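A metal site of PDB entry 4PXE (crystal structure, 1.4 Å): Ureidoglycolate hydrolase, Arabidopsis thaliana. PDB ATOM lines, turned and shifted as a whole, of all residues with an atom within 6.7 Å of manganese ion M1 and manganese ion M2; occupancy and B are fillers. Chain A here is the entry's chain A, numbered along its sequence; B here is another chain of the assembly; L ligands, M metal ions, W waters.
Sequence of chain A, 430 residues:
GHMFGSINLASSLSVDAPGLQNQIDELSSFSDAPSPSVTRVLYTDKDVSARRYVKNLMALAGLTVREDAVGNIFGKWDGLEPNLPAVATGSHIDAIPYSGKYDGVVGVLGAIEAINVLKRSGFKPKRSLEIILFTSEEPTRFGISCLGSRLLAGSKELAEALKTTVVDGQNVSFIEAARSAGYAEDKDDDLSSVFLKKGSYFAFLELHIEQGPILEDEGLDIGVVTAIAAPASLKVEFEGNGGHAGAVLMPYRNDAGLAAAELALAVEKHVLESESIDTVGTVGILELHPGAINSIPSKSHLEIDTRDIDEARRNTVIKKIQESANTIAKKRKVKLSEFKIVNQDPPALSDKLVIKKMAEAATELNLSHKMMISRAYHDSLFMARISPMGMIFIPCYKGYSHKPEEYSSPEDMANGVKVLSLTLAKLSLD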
ATOM      1  N   SER A  91      -5.590   0.808 -27.175  1.00  0.00           N
ATOM      2  CA  SER A  91      -6.369   1.424 -26.111  1.00  0.00           C
ATOM      3  C   SER A  91      -6.723   0.346 -25.086  1.00  0.00           C
ATOM      4  O   SER A  91      -6.108  -0.717 -25.051  1.00  0.00           O
ATOM      5  CB  SER A  91      -7.618   2.100 -26.690  1.00  0.00           C
ATOM      6  OG  SER A  91      -8.168   3.076 -25.813  1.00  0.00           O
ATOM      7  N   HIS A  92      -7.735   0.633 -24.266  1.00  0.00           N
ATOM      8  CA  HIS A  92      -8.100  -0.280 -23.172  1.00  0.00           C
ATOM      9  C   HIS A  92      -9.532  -0.785 -23.341  1.00  0.00           C
ATOM     10  O   HIS A  92     -10.321  -0.194 -24.090  1.00  0.00           O
ATOM     11  CB  HIS A  92      -8.003   0.462 -21.833  1.00  0.00           C
ATOM     12  CG  HIS A  92      -8.958   1.612 -21.726  1.00  0.00           C
ATOM     13  ND1 HIS A  92     -10.143   1.533 -21.037  1.00  0.00           N
ATOM     14  CD2 HIS A  92      -8.904   2.862 -22.259  1.00  0.00           C
ATOM     15  CE1 HIS A  92     -10.788   2.683 -21.146  1.00  0.00           C
ATOM     16  NE2 HIS A  92     -10.054   3.504 -21.873  1.00  0.00           N
ATOM     17  N   ASP A  94     -11.077  -2.085 -20.203  1.00  0.00           N
ATOM     18  CA  ASP A  94     -11.695  -2.029 -18.885  1.00  0.00           C
ATOM     19  C   ASP A  94     -12.668  -0.838 -18.799  1.00  0.00           C
ATOM     20  O   ASP A  94     -12.529   0.137 -19.554  1.00  0.00           O
ATOM     21  CB  ASP A  94     -10.698  -2.135 -17.701  1.00  0.00           C
ATOM     22  CG  ASP A  94      -9.632  -1.034 -17.685  1.00  0.00           C
ATOM     23  OD1 ASP A  94      -9.262  -0.467 -18.736  1.00  0.00           O
ATOM     24  OD2 ASP A  94      -9.098  -0.793 -16.575  1.00  0.00           O
ATOM     25  N   ILE A  96     -15.014   1.490 -15.863  1.00  0.00           N
ATOM     26  CA  ILE A  96     -15.328   1.786 -14.462  1.00  0.00           C
ATOM     27  C   ILE A  96     -16.793   1.450 -14.143  1.00  0.00           C
ATOM     28  O   ILE A  96     -17.603   1.262 -15.044  1.00  0.00           O
ATOM     29  CB  ILE A  96     -14.992   3.258 -14.076  1.00  0.00           C
ATOM     30  CG1 ILE A  96     -16.005   4.247 -14.663  1.00  0.00           C
ATOM     31  CG2 ILE A  96     -13.573   3.609 -14.495  1.00  0.00           C
ATOM     32  CD1 ILE A  96     -15.734   5.676 -14.232  1.00  0.00           C
ATOM     33  N   TYR A 102     -18.144   2.688 -25.082  1.00  0.00           N
ATOM     34  CA  TYR A 102     -17.286   3.253 -26.133  1.00  0.00           C
ATOM     35  C   TYR A 102     -15.900   3.689 -25.655  1.00  0.00           C
ATOM     36  O   TYR A 102     -14.917   3.613 -26.405  1.00  0.00           O
ATOM     37  CB  TYR A 102     -18.011   4.424 -26.840  1.00  0.00           C
ATOM     38  CG  TYR A 102     -19.293   4.012 -27.513  1.00  0.00           C
ATOM     39  CD1 TYR A 102     -19.308   3.615 -28.847  1.00  0.00           C
ATOM     40  CD2 TYR A 102     -20.499   4.021 -26.811  1.00  0.00           C
ATOM     41  CE1 TYR A 102     -20.481   3.220 -29.463  1.00  0.00           C
ATOM     42  CE2 TYR A 102     -21.669   3.627 -27.414  1.00  0.00           C
ATOM     43  CZ  TYR A 102     -21.662   3.226 -28.747  1.00  0.00           C
ATOM     44  OH  TYR A 102     -22.831   2.832 -29.350  1.00  0.00           O
ATOM     45  N   ASP A 103     -15.823   4.123 -24.401  1.00  0.00           N
ATOM     46  CA  ASP A 103     -14.560   4.530 -23.797  1.00  0.00           C
ATOM     47  C   ASP A 103     -13.547   3.382 -23.884  1.00  0.00           C
ATOM     48  O   ASP A 103     -13.823   2.276 -23.440  1.00  0.00           O
ATOM     49  CB  ASP A 103     -14.831   4.927 -22.351  1.00  0.00           C
ATOM     50  CG  ASP A 103     -13.601   5.328 -21.611  1.00  0.00           C
ATOM     51  OD1 ASP A 103     -12.590   5.687 -22.245  1.00  0.00           O
ATOM     52  OD2 ASP A 103     -13.634   5.309 -20.374  1.00  0.00           O
ATOM     53  N   GLY A 104     -12.405   3.644 -24.502  1.00  0.00           N
ATOM     54  CA  GLY A 104     -11.375   2.622 -24.693  1.00  0.00           C
ATOM     55  C   GLY A 104     -11.667   1.622 -25.806  1.00  0.00           C
ATOM     56  O   GLY A 104     -10.838   1.381 -26.703  1.00  0.00           O
ATOM     57  N   VAL A 105     -12.869   1.043 -25.748  1.00  0.00           N
ATOM     58  CA  VAL A 105     -13.237  -0.027 -26.662  1.00  0.00           C
ATOM     59  C   VAL A 105     -13.126   0.396 -28.135  1.00  0.00           C
ATOM     60  O   VAL A 105     -12.652  -0.383 -28.963  1.00  0.00           O
ATOM     61  CB  VAL A 105     -14.655  -0.559 -26.361  1.00  0.00           C
ATOM     62  CG1 VAL A 105     -15.042  -1.635 -27.343  1.00  0.00           C
ATOM     63  CG2 VAL A 105     -14.716  -1.123 -24.941  1.00  0.00           C
ATOM     64  N   GLU A 137      -6.510   0.439 -17.999  1.00  0.00           N
ATOM     65  CA  GLU A 137      -6.209   1.864 -17.984  1.00  0.00           C
ATOM     66  C   GLU A 137      -6.928   2.564 -16.827  1.00  0.00           C
ATOM     67  O   GLU A 137      -6.489   3.617 -16.360  1.00  0.00           O
ATOM     68  CB  GLU A 137      -6.590   2.505 -19.327  1.00  0.00           C
ATOM     69  CG  GLU A 137      -6.222   3.968 -19.459  1.00  0.00           C
ATOM     70  CD  GLU A 137      -7.330   4.914 -19.047  1.00  0.00           C
ATOM     71  OE1 GLU A 137      -8.483   4.465 -18.807  1.00  0.00           O
ATOM     72  OE2 GLU A 137      -7.037   6.126 -18.958  1.00  0.00           O
ATOM     73  N   GLU A 138      -8.048   1.994 -16.387  1.00  0.00           N
ATOM     74  CA  GLU A 138      -8.848   2.623 -15.326  1.00  0.00           C
ATOM     75  C   GLU A 138      -8.308   2.287 -13.938  1.00  0.00           C
ATOM     76  O   GLU A 138      -7.786   1.197 -13.725  1.00  0.00           O
ATOM     77  CB  GLU A 138     -10.311   2.232 -15.460  1.00  0.00           C
ATOM     78  CG  GLU A 138     -10.918   2.619 -16.804  1.00  0.00           C
ATOM     79  CD  GLU A 138     -11.293   4.068 -16.899  1.00  0.00           C
ATOM     80  OE1 GLU A 138     -10.877   4.899 -16.073  1.00  0.00           O
ATOM     81  OE2 GLU A 138     -12.057   4.358 -17.849  1.00  0.00           O
ATOM     82  N   GLU A 206      -3.488   6.597 -30.688  1.00  0.00           N
ATOM     83  CA  GLU A 206      -4.687   6.096 -30.017  1.00  0.00           C
ATOM     84  C   GLU A 206      -5.944   6.767 -30.564  1.00  0.00           C
ATOM     85  O   GLU A 206      -6.060   7.986 -30.550  1.00  0.00           O
ATOM     86  CB  GLU A 206      -4.590   6.336 -28.516  1.00  0.00           C
ATOM     87  CG  GLU A 206      -5.778   5.769 -27.717  1.00  0.00           C
ATOM     88  CD  GLU A 206      -5.541   5.704 -26.213  1.00  0.00           C
ATOM     89  OE1 GLU A 206      -4.527   6.257 -25.713  1.00  0.00           O
ATOM     90  OE2 GLU A 206      -6.379   5.093 -25.526  1.00  0.00           O
ATOM     91  N   HIS A 208      -9.857   7.456 -29.970  1.00  0.00           N
ATOM     92  CA  HIS A 208     -10.653   7.523 -28.742  1.00  0.00           C
ATOM     93  C   HIS A 208     -11.835   8.480 -28.922  1.00  0.00           C
ATOM     94  O   HIS A 208     -11.726   9.476 -29.640  1.00  0.00           O
ATOM     95  CB  HIS A 208      -9.786   7.969 -27.547  1.00  0.00           C
ATOM     96  CG  HIS A 208     -10.299   7.545 -26.202  1.00  0.00           C
ATOM     97  ND1 HIS A 208     -11.414   8.106 -25.613  1.00  0.00           N
ATOM     98  CD2 HIS A 208      -9.860   6.585 -25.342  1.00  0.00           C
ATOM     99  CE1 HIS A 208     -11.636   7.517 -24.440  1.00  0.00           C
ATOM    100  NE2 HIS A 208     -10.707   6.600 -24.257  1.00  0.00           N
ATOM    101  N   ILE A 209     -12.959   8.175 -28.283  1.00  0.00           N
ATOM    102  CA  ILE A 209     -14.038   9.173 -28.253  1.00  0.00           C
ATOM    103  C   ILE A 209     -13.552  10.437 -27.545  1.00  0.00           C
ATOM    104  O   ILE A 209     -12.733  10.380 -26.623  1.00  0.00           O
ATOM    105  CB  ILE A 209     -15.322   8.624 -27.605  1.00  0.00           C
ATOM    106  CG1 ILE A 209     -15.078   8.244 -26.134  1.00  0.00           C
ATOM    107  CG2 ILE A 209     -15.848   7.439 -28.389  1.00  0.00           C
ATOM    108  CD1 ILE A 209     -16.386   7.990 -25.329  1.00  0.00           C
ATOM    109  N   GLN A 211     -14.918  12.437 -25.401  1.00  0.00           N
ATOM    110  CA  GLN A 211     -15.321  12.647 -24.004  1.00  0.00           C
ATOM    111  C   GLN A 211     -15.532  14.131 -23.712  1.00  0.00           C
ATOM    112  O   GLN A 211     -15.317  14.601 -22.590  1.00  0.00           O
ATOM    113  CB  GLN A 211     -14.329  11.996 -23.035  1.00  0.00           C
ATOM    114  CG  GLN A 211     -14.108  10.526 -23.360  1.00  0.00           C
ATOM    115  CD  GLN A 211     -13.134   9.843 -22.428  1.00  0.00           C
ATOM    116  OE1 GLN A 211     -11.932  10.082 -22.493  1.00  0.00           O
ATOM    117  NE2 GLN A 211     -13.647   8.943 -21.594  1.00  0.00           N
ATOM    118  N   ALA A 376      -9.359  14.214 -20.403  1.00  0.00           N
ATOM    119  CA  ALA A 376      -9.136  12.877 -19.883  1.00  0.00           C
ATOM    120  C   ALA A 376      -7.675  12.497 -20.035  1.00  0.00           C
ATOM    121  O   ALA A 376      -6.971  13.035 -20.906  1.00  0.00           O
ATOM    122  CB  ALA A 376     -10.017  11.883 -20.620  1.00  0.00           C
ATOM    123  N   TYR A 377      -7.198  11.576 -19.211  1.00  0.00           N
ATOM    124  CA  TYR A 377      -5.905  10.951 -19.499  1.00  0.00           C
ATOM    125  C   TYR A 377      -6.144   9.652 -20.260  1.00  0.00           C
ATOM    126  O   TYR A 377      -7.288   9.187 -20.398  1.00  0.00           O
ATOM    127  CB  TYR A 377      -5.056  10.745 -18.219  1.00  0.00           C
ATOM    128  CG  TYR A 377      -5.744   9.958 -17.123  1.00  0.00           C
ATOM    129  CD1 TYR A 377      -6.333  10.604 -16.021  1.00  0.00           C
ATOM    130  CD2 TYR A 377      -5.829   8.576 -17.183  1.00  0.00           C
ATOM    131  CE1 TYR A 377      -6.980   9.877 -15.024  1.00  0.00           C
ATOM    132  CE2 TYR A 377      -6.467   7.845 -16.203  1.00  0.00           C
ATOM    133  CZ  TYR A 377      -7.033   8.484 -15.121  1.00  0.00           C
ATOM    134  OH  TYR A 377      -7.677   7.742 -14.153  1.00  0.00           O
ATOM    135  N   HIS A 378      -5.060   9.094 -20.796  1.00  0.00           N
ATOM    136  CA  HIS A 378      -5.123   7.921 -21.656  1.00  0.00           C
ATOM    137  C   HIS A 378      -3.799   7.200 -21.575  1.00  0.00           C
ATOM    138  O   HIS A 378      -2.810   7.771 -21.128  1.00  0.00           O
ATOM    139  CB  HIS A 378      -5.307   8.352 -23.118  1.00  0.00           C
ATOM    140  CG  HIS A 378      -6.531   9.183 -23.371  1.00  0.00           C
ATOM    141  ND1 HIS A 378      -7.781   8.634 -23.523  1.00  0.00           N
ATOM    142  CD2 HIS A 378      -6.678  10.518 -23.521  1.00  0.00           C
ATOM    143  CE1 HIS A 378      -8.647   9.602 -23.766  1.00  0.00           C
ATOM    144  NE2 HIS A 378      -8.008  10.754 -23.765  1.00  0.00           N
ATOM    145  N   ASP A 379      -3.755   5.967 -22.069  1.00  0.00           N
ATOM    146  CA  ASP A 379      -2.476   5.271 -22.228  1.00  0.00           C
ATOM    147  C   ASP A 379      -1.464   6.053 -23.062  1.00  0.00           C
ATOM    148  O   ASP A 379      -0.259   5.942 -22.838  1.00  0.00           O
ATOM    149  CB  ASP A 379      -2.719   3.884 -22.818  1.00  0.00           C
ATOM    150  CG  ASP A 379      -3.466   2.979 -21.842  1.00  0.00           C
ATOM    151  OD1 ASP A 379      -2.903   2.738 -20.757  1.00  0.00           O
ATOM    152  OD2 ASP A 379      -4.596   2.539 -22.142  1.00  0.00           O
ATOM    153  N   SER A 401     -19.532  10.772 -20.983  1.00  0.00           N
ATOM    154  CA  SER A 401     -18.660   9.618 -20.807  1.00  0.00           C
ATOM    155  C   SER A 401     -18.675   9.196 -19.340  1.00  0.00           C
ATOM    156  O   SER A 401     -19.120   9.945 -18.466  1.00  0.00           O
ATOM    157  CB  SER A 401     -17.243   9.926 -21.309  1.00  0.00           C
ATOM    158  OG  SER A 401     -16.483   8.748 -21.446  1.00  0.00           O
ATOM    159  N   HIS A 402     -18.212   7.981 -19.070  1.00  0.00           N
ATOM    160  CA  HIS A 402     -18.256   7.382 -17.726  1.00  0.00           C
ATOM    161  C   HIS A 402     -19.678   7.275 -17.196  1.00  0.00           C
ATOM    162  O   HIS A 402     -19.931   7.364 -16.001  1.00  0.00           O
ATOM    163  CB  HIS A 402     -17.365   8.152 -16.752  1.00  0.00           C
ATOM    164  CG  HIS A 402     -15.910   7.835 -16.899  1.00  0.00           C
ATOM    165  ND1 HIS A 402     -14.934   8.389 -16.093  1.00  0.00           N
ATOM    166  CD2 HIS A 402     -15.268   7.017 -17.765  1.00  0.00           C
ATOM    167  CE1 HIS A 402     -13.758   7.921 -16.449  1.00  0.00           C
ATOM    168  NE2 HIS A 402     -13.930   7.088 -17.456  1.00  0.00           N
ATOM    169  N   GLU A 406     -23.223   7.557 -22.728  1.00  0.00           N
ATOM    170  CA  GLU A 406     -22.111   7.645 -23.670  1.00  0.00           C
ATOM    171  C   GLU A 406     -22.496   7.039 -25.027  1.00  0.00           C
ATOM    172  O   GLU A 406     -23.034   5.941 -25.092  1.00  0.00           O
ATOM    173  CB  GLU A 406     -20.905   6.906 -23.088  1.00  0.00           C
ATOM    174  CG  GLU A 406     -19.625   6.958 -23.904  1.00  0.00           C
ATOM    175  CD  GLU A 406     -18.546   6.168 -23.215  1.00  0.00           C
ATOM    176  OE1 GLU A 406     -18.442   4.962 -23.507  1.00  0.00           O
ATOM    177  OE2 GLU A 406     -17.854   6.736 -22.335  1.00  0.00           O
ATOM    178  N   HIS B 244     -17.840  12.371 -16.480  1.00  0.00           N
ATOM    179  CA  HIS B 244     -16.400  12.188 -16.436  1.00  0.00           C
ATOM    180  C   HIS B 244     -15.717  13.241 -15.567  1.00  0.00           C
ATOM    181  O   HIS B 244     -15.806  14.435 -15.824  1.00  0.00           O
ATOM    182  CB  HIS B 244     -15.864  12.266 -17.868  1.00  0.00           C
ATOM    183  CG  HIS B 244     -14.521  11.662 -18.016  1.00  0.00           C
ATOM    184  ND1 HIS B 244     -13.382  12.218 -17.471  1.00  0.00           N
ATOM    185  CD2 HIS B 244     -14.105  10.538 -18.672  1.00  0.00           C
ATOM    186  CE1 HIS B 244     -12.338  11.475 -17.772  1.00  0.00           C
ATOM    187  NE2 HIS B 244     -12.744  10.441 -18.494  1.00  0.00           N
ATOM    188  N   ASN B 294     -12.951   8.558 -10.623  1.00  0.00           N
ATOM    189  CA  ASN B 294     -13.005   9.395 -11.812  1.00  0.00           C
ATOM    190  C   ASN B 294     -14.408   9.497 -12.435  1.00  0.00           C
ATOM    191  O   ASN B 294     -14.572   9.786 -13.640  1.00  0.00           O
ATOM    192  CB  ASN B 294     -11.940   8.955 -12.833  1.00  0.00           C
ATOM    193  CG  ASN B 294     -11.991   7.464 -13.173  1.00  0.00           C
ATOM    194  OD1 ASN B 294     -12.615   6.659 -12.471  1.00  0.00           O
ATOM    195  ND2 ASN B 294     -11.311   7.091 -14.259  1.00  0.00           N
HETATM  196  C1  LIG L   1      -9.603   7.826 -17.446  1.00  0.00           C
HETATM  197  O1  LIG L   1      -8.914   7.753 -18.650  1.00  0.00           O
HETATM  198  C2  LIG L   1      -9.820   9.208 -16.945  1.00  0.00           C
HETATM  199  O2  LIG L   1      -9.392  10.187 -17.636  1.00  0.00           O
HETATM  200  O3  LIG L   1     -10.422   9.392 -15.850  1.00  0.00           O
HETATM  201 MN    MN M   1     -10.406   5.761 -22.113  1.00  0.00          MN
HETATM  202 MN    MN M   2     -12.308   6.245 -18.875  1.00  0.00          MN
HETATM  203  O   HOH W   1     -12.113   7.964 -19.460  1.00  0.00           O
HETATM  204  O   HOH W   2      -8.225   6.140 -22.376  1.00  0.00           O
HETATM  205  O   HOH W   3     -10.488   5.751 -19.887  1.00  0.00           O
HETATM  206  O   HOH W   4     -10.226   8.147 -21.461  1.00  0.00           O
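OE2 of Glu 137 sits close to O1 of the ligand (2.5 Å).
A ring nitrogen (NE2) of His 244 of chain B sits close to an oxygen (O2) of the ligand (3.5 Å).
O3 of the ligand lies within hydrogen-bond range of ND2 of Asn 294 of chain B (2.9 Å).
N of Tyr 377 is in hydrogen-bond range of O2 of the ligand.
The side-chain carboxylate (OE1) of Glu 138 sits at hydrogen-bond distance from the side-chain amide nitrogen (ND2) of Asn 294 of chain B, at 2.9 Å.
NE2 of Gln 211 lies close to OD1 of Asp 103, 3.5 Å away.
OE1 of Glu 406 sits at hydrogen-bond distance from N of Asp 103 (2.9 Å).
ND1 of His 92 sits at hydrogen-bond distance from O of Asp 94, at 3.1 Å.
N of Val 105 sits at hydrogen-bond distance from O of His 92 (3.3 Å).
The backbone carbonyl oxygen (O) of Asn 294 of chain B is in hydrogen-bond range of a ring nitrogen (ND1) of His 402, 2.8 Å away.
NE2 of His 208 lies close to N of Gly 104, 3.4 Å away.
The backbone carbonyl oxygen (O) of Gly 104 sits at hydrogen-bond distance from the side-chain hydroxyl (OG) of Ser 91.
Gly 104 touches manganese ion M1.
Of the 23 residues printed, 4 come within 4 Å of manganese ion M1.
Three residues have an atom within 4 Å of manganese ion M2: Asp 103, Glu 138 and His 402.
The nearest printed residue that does not touch manganese ion M2 is Gln 211 (4.1 Å).
Manganese ion M1 is bound by the side-chain carboxylate of Asp 103, water W3, water W2, a ring nitrogen (NE2) of His 92, a ring nitrogen (NE2) of His 208 and water W4.
Manganese ion M1 has six donor atoms within binding distance.
Water W1 is bound to manganese ion M2, at 1.8 Å.
Water W3 binds manganese ion M2.
The side-chain carboxylate (OE2) of Glu 138 is bound to manganese ion M2 (2.2 Å).
Manganese ion M2 is bound by the side-chain carboxylate (OD2) of Asp 103, 2.2 Å away.
Manganese ion M2 is bound by NE2 of His 402 (2.3 Å).
Manganese ion M2 has five donor atoms within binding distance.
Water W3 lies within hydrogen-bond range of OE1 of Glu 137 (2.6 Å) and O1 of the ligand (2.8 Å).
Water W1 lies within hydrogen-bond range of a ring nitrogen (NE2) of His 244 of chain B (2.7 Å), the side-chain amide nitrogen (NE2) of Gln 211 (2.8 Å) and an oxygen (O1) of the ligand (3.3 Å).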
